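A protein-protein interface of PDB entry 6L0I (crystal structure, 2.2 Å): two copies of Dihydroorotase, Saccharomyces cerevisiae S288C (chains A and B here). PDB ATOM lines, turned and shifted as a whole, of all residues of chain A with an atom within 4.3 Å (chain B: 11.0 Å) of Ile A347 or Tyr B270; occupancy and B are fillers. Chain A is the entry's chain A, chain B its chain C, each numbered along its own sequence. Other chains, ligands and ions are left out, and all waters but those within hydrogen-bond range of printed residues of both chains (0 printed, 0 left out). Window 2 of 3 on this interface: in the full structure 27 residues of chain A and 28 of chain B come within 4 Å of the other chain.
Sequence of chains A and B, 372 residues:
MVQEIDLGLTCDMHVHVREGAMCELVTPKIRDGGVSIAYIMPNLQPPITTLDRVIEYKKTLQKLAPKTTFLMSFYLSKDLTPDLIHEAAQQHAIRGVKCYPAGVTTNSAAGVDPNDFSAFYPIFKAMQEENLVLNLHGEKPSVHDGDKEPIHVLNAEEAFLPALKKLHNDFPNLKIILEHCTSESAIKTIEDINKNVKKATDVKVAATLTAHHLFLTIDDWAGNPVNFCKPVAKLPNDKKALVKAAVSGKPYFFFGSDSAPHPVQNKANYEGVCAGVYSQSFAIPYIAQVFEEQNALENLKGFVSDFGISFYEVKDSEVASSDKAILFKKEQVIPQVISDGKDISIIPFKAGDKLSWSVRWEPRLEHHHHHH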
ATOM      1  N   ASN A 224     -32.394  -9.343  11.413  1.00  0.00           N
ATOM      2  CA  ASN A 224     -31.936  -7.990  11.743  1.00  0.00           C
ATOM      3  C   ASN A 224     -32.969  -7.304  12.624  1.00  0.00           C
ATOM      4  O   ASN A 224     -33.911  -6.674  12.121  1.00  0.00           O
ATOM      5  CB  ASN A 224     -31.684  -7.150  10.490  1.00  0.00           C
ATOM      6  CG  ASN A 224     -30.562  -7.696   9.618  1.00  0.00           C
ATOM      7  OD1 ASN A 224     -29.427  -7.890  10.066  1.00  0.00           O
ATOM      8  ND2 ASN A 224     -30.880  -7.936   8.350  1.00  0.00           N
ATOM      9  N   PRO A 225     -32.821  -7.403  13.950  1.00  0.00           N
ATOM     10  CA  PRO A 225     -33.775  -6.756  14.869  1.00  0.00           C
ATOM     11  C   PRO A 225     -33.923  -5.238  14.706  1.00  0.00           C
ATOM     12  O   PRO A 225     -34.984  -4.697  15.037  1.00  0.00           O
ATOM     13  CB  PRO A 225     -33.197  -7.108  16.244  1.00  0.00           C
ATOM     14  CG  PRO A 225     -32.479  -8.400  16.020  1.00  0.00           C
ATOM     15  CD  PRO A 225     -31.912  -8.330  14.647  1.00  0.00           C
ATOM     16  N   VAL A 226     -32.891  -4.526  14.242  1.00  0.00           N
ATOM     17  CA  VAL A 226     -33.044  -3.090  14.006  1.00  0.00           C
ATOM     18  C   VAL A 226     -34.163  -2.816  13.017  1.00  0.00           C
ATOM     19  O   VAL A 226     -34.768  -1.738  13.043  1.00  0.00           O
ATOM     20  CB  VAL A 226     -31.735  -2.450  13.501  1.00  0.00           C
ATOM     21  CG1 VAL A 226     -30.807  -2.165  14.647  1.00  0.00           C
ATOM     22  CG2 VAL A 226     -31.081  -3.310  12.405  1.00  0.00           C
ATOM     23  N   VAL A 264     -30.123   0.816  21.978  1.00  0.00           N
ATOM     24  CA  VAL A 264     -29.572  -0.336  21.272  1.00  0.00           C
ATOM     25  C   VAL A 264     -29.577  -1.612  22.122  1.00  0.00           C
ATOM     26  O   VAL A 264     -29.629  -2.716  21.571  1.00  0.00           O
ATOM     27  CB  VAL A 264     -28.153   0.022  20.766  1.00  0.00           C
ATOM     28  CG1 VAL A 264     -27.175   0.154  21.931  1.00  0.00           C
ATOM     29  CG2 VAL A 264     -27.662  -0.987  19.756  1.00  0.00           C
ATOM     30  N   LYS A 267     -32.609  -3.685  21.459  1.00  0.00           N
ATOM     31  CA  LYS A 267     -32.650  -4.399  20.195  1.00  0.00           C
ATOM     32  C   LYS A 267     -31.768  -5.639  20.189  1.00  0.00           C
ATOM     33  O   LYS A 267     -32.131  -6.638  19.561  1.00  0.00           O
ATOM     34  CB  LYS A 267     -32.239  -3.473  19.052  1.00  0.00           C
ATOM     35  CG  LYS A 267     -33.256  -2.392  18.787  1.00  0.00           C
ATOM     36  CD  LYS A 267     -34.488  -3.050  18.244  1.00  0.00           C
ATOM     37  CE  LYS A 267     -35.388  -2.067  17.574  1.00  0.00           C
ATOM     38  NZ  LYS A 267     -36.201  -2.763  16.560  1.00  0.00           N
ATOM     39  N   ALA A 268     -30.633  -5.610  20.888  1.00  0.00           N
ATOM     40  CA  ALA A 268     -29.729  -6.763  20.967  1.00  0.00           C
ATOM     41  C   ALA A 268     -30.149  -7.669  22.123  1.00  0.00           C
ATOM     42  O   ALA A 268     -29.461  -7.822  23.130  1.00  0.00           O
ATOM     43  CB  ALA A 268     -28.287  -6.303  21.124  1.00  0.00           C
ATOM     44  N   TYR A 278     -36.280   3.620  14.069  1.00  0.00           N
ATOM     45  CA  TYR A 278     -36.045   5.035  14.354  1.00  0.00           C
ATOM     46  C   TYR A 278     -35.676   5.738  13.061  1.00  0.00           C
ATOM     47  O   TYR A 278     -34.561   5.566  12.562  1.00  0.00           O
ATOM     48  CB  TYR A 278     -34.931   5.242  15.378  1.00  0.00           C
ATOM     49  CG  TYR A 278     -34.583   6.712  15.540  1.00  0.00           C
ATOM     50  CD1 TYR A 278     -35.474   7.584  16.153  1.00  0.00           C
ATOM     51  CD2 TYR A 278     -33.384   7.231  15.056  1.00  0.00           C
ATOM     52  CE1 TYR A 278     -35.191   8.922  16.290  1.00  0.00           C
ATOM     53  CE2 TYR A 278     -33.087   8.581  15.186  1.00  0.00           C
ATOM     54  CZ  TYR A 278     -34.001   9.419  15.808  1.00  0.00           C
ATOM     55  OH  TYR A 278     -33.733  10.754  15.958  1.00  0.00           O
ATOM     56  N   GLN A 336     -23.710   5.521  12.030  1.00  0.00           N
ATOM     57  CA  GLN A 336     -23.907   4.189  12.588  1.00  0.00           C
ATOM     58  C   GLN A 336     -24.718   4.246  13.866  1.00  0.00           C
ATOM     59  O   GLN A 336     -25.379   3.266  14.220  1.00  0.00           O
ATOM     60  CB  GLN A 336     -22.561   3.516  12.872  1.00  0.00           C
ATOM     61  CG  GLN A 336     -21.620   3.441  11.674  1.00  0.00           C
ATOM     62  CD  GLN A 336     -22.095   2.446  10.635  1.00  0.00           C
ATOM     63  OE1 GLN A 336     -22.844   1.516  10.946  1.00  0.00           O
ATOM     64  NE2 GLN A 336     -21.661   2.632   9.391  1.00  0.00           N
ATOM     65  N   ILE A 346     -28.878   5.089  19.731  1.00  0.00           N
ATOM     66  CA  ILE A 346     -29.882   4.533  18.829  1.00  0.00           C
ATOM     67  C   ILE A 346     -29.199   4.142  17.540  1.00  0.00           C
ATOM     68  O   ILE A 346     -28.364   4.897  17.030  1.00  0.00           O
ATOM     69  CB  ILE A 346     -31.016   5.509  18.458  1.00  0.00           C
ATOM     70  CG1 ILE A 346     -31.623   6.230  19.640  1.00  0.00           C
ATOM     71  CG2 ILE A 346     -32.091   4.812  17.614  1.00  0.00           C
ATOM     72  CD1 ILE A 346     -32.174   7.546  19.145  1.00  0.00           C
ATOM     73  N   ILE A 347     -29.617   3.014  16.972  1.00  0.00           N
ATOM     74  CA  ILE A 347     -29.297   2.667  15.591  1.00  0.00           C
ATOM     75  C   ILE A 347     -30.368   3.283  14.695  1.00  0.00           C
ATOM     76  O   ILE A 347     -31.544   2.912  14.817  1.00  0.00           O
ATOM     77  CB  ILE A 347     -29.233   1.151  15.392  1.00  0.00           C
ATOM     78  CG1 ILE A 347     -28.477   0.492  16.556  1.00  0.00           C
ATOM     79  CG2 ILE A 347     -28.631   0.831  14.034  1.00  0.00           C
ATOM     80  CD1 ILE A 347     -27.047   0.967  16.714  1.00  0.00           C
ATOM     81  N   PRO A 348     -30.025   4.219  13.819  1.00  0.00           N
ATOM     82  CA  PRO A 348     -31.026   4.783  12.912  1.00  0.00           C
ATOM     83  C   PRO A 348     -31.274   3.872  11.717  1.00  0.00           C
ATOM     84  O   PRO A 348     -30.454   3.022  11.363  1.00  0.00           O
ATOM     85  CB  PRO A 348     -30.392   6.107  12.474  1.00  0.00           C
ATOM     86  CG  PRO A 348     -28.921   5.823  12.518  1.00  0.00           C
ATOM     87  CD  PRO A 348     -28.727   4.911  13.710  1.00  0.00           C
ATOM     88  N   PHE A 349     -32.443   4.066  11.105  1.00  0.00           N
ATOM     89  CA  PHE A 349     -32.838   3.323   9.913  1.00  0.00           C
ATOM     90  C   PHE A 349     -31.814   3.501   8.797  1.00  0.00           C
ATOM     91  O   PHE A 349     -31.384   4.620   8.511  1.00  0.00           O
ATOM     92  CB  PHE A 349     -34.210   3.813   9.454  1.00  0.00           C
ATOM     93  CG  PHE A 349     -34.724   3.146   8.215  1.00  0.00           C
ATOM     94  CD1 PHE A 349     -34.729   1.759   8.099  1.00  0.00           C
ATOM     95  CD2 PHE A 349     -35.240   3.903   7.184  1.00  0.00           C
ATOM     96  CE1 PHE A 349     -35.211   1.142   6.960  1.00  0.00           C
ATOM     97  CE2 PHE A 349     -35.726   3.302   6.032  1.00  0.00           C
ATOM     98  CZ  PHE A 349     -35.716   1.922   5.917  1.00  0.00           C
ATOM     99  N   ALA A 351     -28.716   2.726   8.736  1.00  0.00           N
ATOM    100  CA  ALA A 351     -27.452   3.235   9.260  1.00  0.00           C
ATOM    101  C   ALA A 351     -26.289   2.889   8.336  1.00  0.00           C
ATOM    102  O   ALA A 351     -26.208   1.779   7.804  1.00  0.00           O
ATOM    103  CB  ALA A 351     -27.190   2.669  10.659  1.00  0.00           C
ATOM    104  N   GLY B 223     -39.495 -11.283  16.542  1.00  0.00           N
ATOM    105  CA  GLY B 223     -39.117 -10.702  17.809  1.00  0.00           C
ATOM    106  C   GLY B 223     -38.333 -11.592  18.752  1.00  0.00           C
ATOM    107  O   GLY B 223     -38.082 -11.177  19.889  1.00  0.00           O
ATOM    108  N   PRO B 225     -34.910 -13.775  18.288  1.00  0.00           N
ATOM    109  CA  PRO B 225     -33.816 -14.389  17.526  1.00  0.00           C
ATOM    110  C   PRO B 225     -33.465 -15.795  17.965  1.00  0.00           C
ATOM    111  O   PRO B 225     -32.999 -16.583  17.134  1.00  0.00           O
ATOM    112  CB  PRO B 225     -32.653 -13.411  17.750  1.00  0.00           C
ATOM    113  CG  PRO B 225     -33.346 -12.066  17.928  1.00  0.00           C
ATOM    114  CD  PRO B 225     -34.607 -12.379  18.673  1.00  0.00           C
ATOM    115  N   PHE B 228     -34.976 -18.044  15.628  1.00  0.00           N
ATOM    116  CA  PHE B 228     -34.725 -17.750  14.221  1.00  0.00           C
ATOM    117  C   PHE B 228     -33.742 -18.778  13.672  1.00  0.00           C
ATOM    118  O   PHE B 228     -32.637 -18.928  14.202  1.00  0.00           O
ATOM    119  CB  PHE B 228     -34.177 -16.334  14.050  1.00  0.00           C
ATOM    120  CG  PHE B 228     -33.662 -16.040  12.674  1.00  0.00           C
ATOM    121  CD1 PHE B 228     -34.494 -16.099  11.575  1.00  0.00           C
ATOM    122  CD2 PHE B 228     -32.349 -15.689  12.482  1.00  0.00           C
ATOM    123  CE1 PHE B 228     -34.000 -15.823  10.291  1.00  0.00           C
ATOM    124  CE2 PHE B 228     -31.849 -15.411  11.219  1.00  0.00           C
ATOM    125  CZ  PHE B 228     -32.661 -15.473  10.124  1.00  0.00           C
ATOM    126  N   VAL B 264     -24.736 -17.436  22.982  1.00  0.00           N
ATOM    127  CA  VAL B 264     -25.842 -16.497  23.195  1.00  0.00           C
ATOM    128  C   VAL B 264     -25.524 -15.101  22.675  1.00  0.00           C
ATOM    129  O   VAL B 264     -26.428 -14.370  22.244  1.00  0.00           O
ATOM    130  CB  VAL B 264     -26.215 -16.439  24.694  1.00  0.00           C
ATOM    131  CG1 VAL B 264     -25.055 -15.880  25.527  1.00  0.00           C
ATOM    132  CG2 VAL B 264     -27.451 -15.589  24.907  1.00  0.00           C
ATOM    133  N   GLN B 265     -24.258 -14.690  22.714  1.00  0.00           N
ATOM    134  CA  GLN B 265     -23.945 -13.353  22.223  1.00  0.00           C
ATOM    135  C   GLN B 265     -24.031 -13.282  20.709  1.00  0.00           C
ATOM    136  O   GLN B 265     -24.204 -12.185  20.165  1.00  0.00           O
ATOM    137  CB  GLN B 265     -22.566 -12.892  22.719  1.00  0.00           C
ATOM    138  CG  GLN B 265     -21.363 -13.644  22.135  1.00  0.00           C
ATOM    139  CD  GLN B 265     -20.916 -14.835  22.995  1.00  0.00           C
ATOM    140  OE1 GLN B 265     -21.649 -15.307  23.891  1.00  0.00           O
ATOM    141  NE2 GLN B 265     -19.706 -15.329  22.722  1.00  0.00           N
ATOM    142  N   ASN B 266     -23.955 -14.418  20.009  1.00  0.00           N
ATOM    143  CA  ASN B 266     -24.254 -14.384  18.583  1.00  0.00           C
ATOM    144  C   ASN B 266     -25.751 -14.396  18.272  1.00  0.00           C
ATOM    145  O   ASN B 266     -26.120 -14.175  17.118  1.00  0.00           O
ATOM    146  CB  ASN B 266     -23.561 -15.536  17.859  1.00  0.00           C
ATOM    147  CG  ASN B 266     -22.070 -15.304  17.716  1.00  0.00           C
ATOM    148  OD1 ASN B 266     -21.567 -14.234  18.059  1.00  0.00           O
ATOM    149  ND2 ASN B 266     -21.357 -16.305  17.219  1.00  0.00           N
ATOM    150  N   LYS B 267     -26.630 -14.612  19.250  1.00  0.00           N
ATOM    151  CA  LYS B 267     -28.066 -14.468  19.001  1.00  0.00           C
ATOM    152  C   LYS B 267     -28.625 -13.120  19.430  1.00  0.00           C
ATOM    153  O   LYS B 267     -29.688 -12.719  18.937  1.00  0.00           O
ATOM    154  CB  LYS B 267     -28.867 -15.558  19.726  1.00  0.00           C
ATOM    155  CG  LYS B 267     -28.455 -17.003  19.417  1.00  0.00           C
ATOM    156  CD  LYS B 267     -28.653 -17.355  17.947  1.00  0.00           C
ATOM    157  CE  LYS B 267     -30.118 -17.399  17.599  1.00  0.00           C
ATOM    158  NZ  LYS B 267     -30.410 -18.098  16.306  1.00  0.00           N
ATOM    159  N   ALA B 268     -27.964 -12.426  20.350  1.00  0.00           N
ATOM    160  CA  ALA B 268     -28.440 -11.131  20.835  1.00  0.00           C
ATOM    161  C   ALA B 268     -27.648 -10.000  20.186  1.00  0.00           C
ATOM    162  O   ALA B 268     -26.956  -9.239  20.854  1.00  0.00           O
ATOM    163  CB  ALA B 268     -28.349 -11.072  22.354  1.00  0.00           C
ATOM    164  N   ASN B 269     -27.713  -9.965  18.854  1.00  0.00           N
ATOM    165  CA  ASN B 269     -27.198  -8.897  18.006  1.00  0.00           C
ATOM    166  C   ASN B 269     -28.366  -8.020  17.589  1.00  0.00           C
ATOM    167  O   ASN B 269     -29.489  -8.501  17.457  1.00  0.00           O
ATOM    168  CB  ASN B 269     -26.537  -9.420  16.718  1.00  0.00           C
ATOM    169  CG  ASN B 269     -25.422 -10.424  16.963  1.00  0.00           C
ATOM    170  OD1 ASN B 269     -25.296 -10.962  18.055  1.00  0.00           O
ATOM    171  ND2 ASN B 269     -24.606 -10.690  15.922  1.00  0.00           N
ATOM    172  N   TYR B 270     -28.105  -6.738  17.347  1.00  0.00           N
ATOM    173  CA  TYR B 270     -29.163  -5.948  16.736  1.00  0.00           C
ATOM    174  C   TYR B 270     -29.160  -6.041  15.216  1.00  0.00           C
ATOM    175  O   TYR B 270     -30.144  -5.646  14.582  1.00  0.00           O
ATOM    176  CB  TYR B 270     -29.093  -4.483  17.190  1.00  0.00           C
ATOM    177  CG  TYR B 270     -27.853  -3.714  16.795  1.00  0.00           C
ATOM    178  CD1 TYR B 270     -26.844  -3.489  17.712  1.00  0.00           C
ATOM    179  CD2 TYR B 270     -27.703  -3.191  15.518  1.00  0.00           C
ATOM    180  CE1 TYR B 270     -25.716  -2.773  17.374  1.00  0.00           C
ATOM    181  CE2 TYR B 270     -26.574  -2.482  15.166  1.00  0.00           C
ATOM    182  CZ  TYR B 270     -25.588  -2.270  16.111  1.00  0.00           C
ATOM    183  OH  TYR B 270     -24.456  -1.561  15.804  1.00  0.00           O
ATOM    184  N   GLU B 271     -28.099  -6.573  14.624  1.00  0.00           N
ATOM    185  CA  GLU B 271     -28.061  -6.861  13.199  1.00  0.00           C
ATOM    186  C   GLU B 271     -27.279  -8.145  12.988  1.00  0.00           C
ATOM    187  O   GLU B 271     -26.380  -8.473  13.764  1.00  0.00           O
ATOM    188  CB  GLU B 271     -27.408  -5.730  12.407  1.00  0.00           C
ATOM    189  CG  GLU B 271     -25.948  -5.524  12.770  1.00  0.00           C
ATOM    190  CD  GLU B 271     -25.330  -4.337  12.063  1.00  0.00           C
ATOM    191  OE1 GLU B 271     -25.589  -4.159  10.848  1.00  0.00           O
ATOM    192  OE2 GLU B 271     -24.588  -3.579  12.729  1.00  0.00           O
ATOM    193  N   GLY B 272     -27.617  -8.862  11.924  1.00  0.00           N
ATOM    194  CA  GLY B 272     -26.910 -10.097  11.612  1.00  0.00           C
ATOM    195  C   GLY B 272     -26.968 -11.160  12.693  1.00  0.00           C
ATOM    196  O   GLY B 272     -25.942 -11.786  12.998  1.00  0.00           O
ATOM    197  N   VAL B 273     -28.147 -11.363  13.295  1.00  0.00           N
ATOM    198  CA  VAL B 273     -28.373 -12.533  14.136  1.00  0.00           C
ATOM    199  C   VAL B 273     -27.992 -13.787  13.381  1.00  0.00           C
ATOM    200  O   VAL B 273     -28.353 -13.953  12.213  1.00  0.00           O
ATOM    201  CB  VAL B 273     -29.846 -12.605  14.577  1.00  0.00           C
ATOM    202  CG1 VAL B 273     -30.124 -13.958  15.261  1.00  0.00           C
ATOM    203  CG2 VAL B 273     -30.187 -11.427  15.483  1.00  0.00           C
ATOM    204  N   CYS B 274     -27.253 -14.674  14.045  1.00  0.00           N
ATOM    205  CA  CYS B 274     -26.966 -15.993  13.490  1.00  0.00           C
ATOM    206  C   CYS B 274     -28.212 -16.869  13.513  1.00  0.00           C
ATOM    207  O   CYS B 274     -28.915 -16.933  14.529  1.00  0.00           O
ATOM    208  CB  CYS B 274     -25.861 -16.676  14.302  1.00  0.00           C
ATOM    209  SG  CYS B 274     -24.238 -15.923  14.121  1.00  0.00           S
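Ala A268 touches its own counterpart, Ala B268.
C of Asn A224 touches O of Tyr B270, 3.8 Å away. Glu B271 touches Asn A224 (CA to OD1, 3.6 Å). Pro A225 touches Asn B269. CD of Pro A225 touches CG2 of Val B273 (3.6 Å). Tyr B270 touches Val A264 (CD1 to CG2, 3.3 Å). Asn B269 touches Lys A267 (O to O, 3.9 Å). CB of Tyr B270 touches CB of Lys A267, at 3.8 Å. CA of Ala A268 touches C of Asn B269 (3.9 Å). Ala A268 touches Tyr B270 (CB to N, 3.8 Å). Ile A347 touches Tyr B270.
O of Tyr B270 lies close to N of Pro A225. N of Val A226 is in hydrogen-bond range of O of Tyr B270 (3.0 Å). N of Gly B272 is in hydrogen-bond range of OD1 of Asn A224 (2.8 Å).
Of the 13 printed residues of chain A, 7 touch a printed residue of chain B. Hydrophobic or aromatic side chains of chain A that line the printed part of chain B: Pro A225, Val A226, Val A264, Ala A268 and Ile A347. Hydrophobic or aromatic side chains of chain B that line the printed part of chain A: Ala B268, Tyr B270 and Val B273.
Of chain B, only Tyr B270 (3.8 Å), Glu B271 (3.6 Å) and Gly B272 (2.8 Å) come within 4 Å of Asn A224. Of chain B, only Asn B269 (3.3 Å), Tyr B270 (3.2 Å) and Val B273 (3.6 Å) come within 4 Å of Pro A225. Of chain B, only Tyr B270 comes within 4 Å of Val A264. No residue of chain B comes within 4 Å of Ile A346. Of the printed residues of chain B, Ile A347 touches Tyr B270 (3.6 Å). No residue of chain B comes within 4 Å of Pro A348. No residue of chain B comes within 4 Å of Ala A351. Pro B225 touches none of the printed residues of chain A. Lys B267 touches none of the printed residues of chain A. Printed residues of chain A within 4 Å of Ala B268: Ala A268 (3.2 Å). Printed residues of chain A within 4 Å of Asn B269: Pro A225 (3.3 Å), Lys A267 (3.9 Å) and Ala A268 (3.9 Å). Tyr B270 touches seven residues of chain A. Printed residues of chain A within 4 Å of Glu B271: Asn A224. Printed residues of chain A within 4 Å of Val B273: Pro A225 (3.6 Å). The nearest residue of chain B that does not touch Ile A347 is Glu B271 (6.1 Å). The nearest printed residue of chain A that does not touch Tyr B270 is Gln A336 (5.2 Å).
O of Gln B265 sits close to OD1 of Asn B269, 2.7 Å away. The side-chain amide nitrogen (ND2) of Asn B269 is in hydrogen-bond range of the backbone carbonyl oxygen (O) of Gly B272, 3.4 Å away. O of Pro A225 is in hydrogen-bond range of NZ of Lys A267, 2.7 Å away. The backbone carbonyl oxygen (O) of Asn B266 sits close to the side-chain amide oxygen (OD1) of Asn B269, 3.4 Å away.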
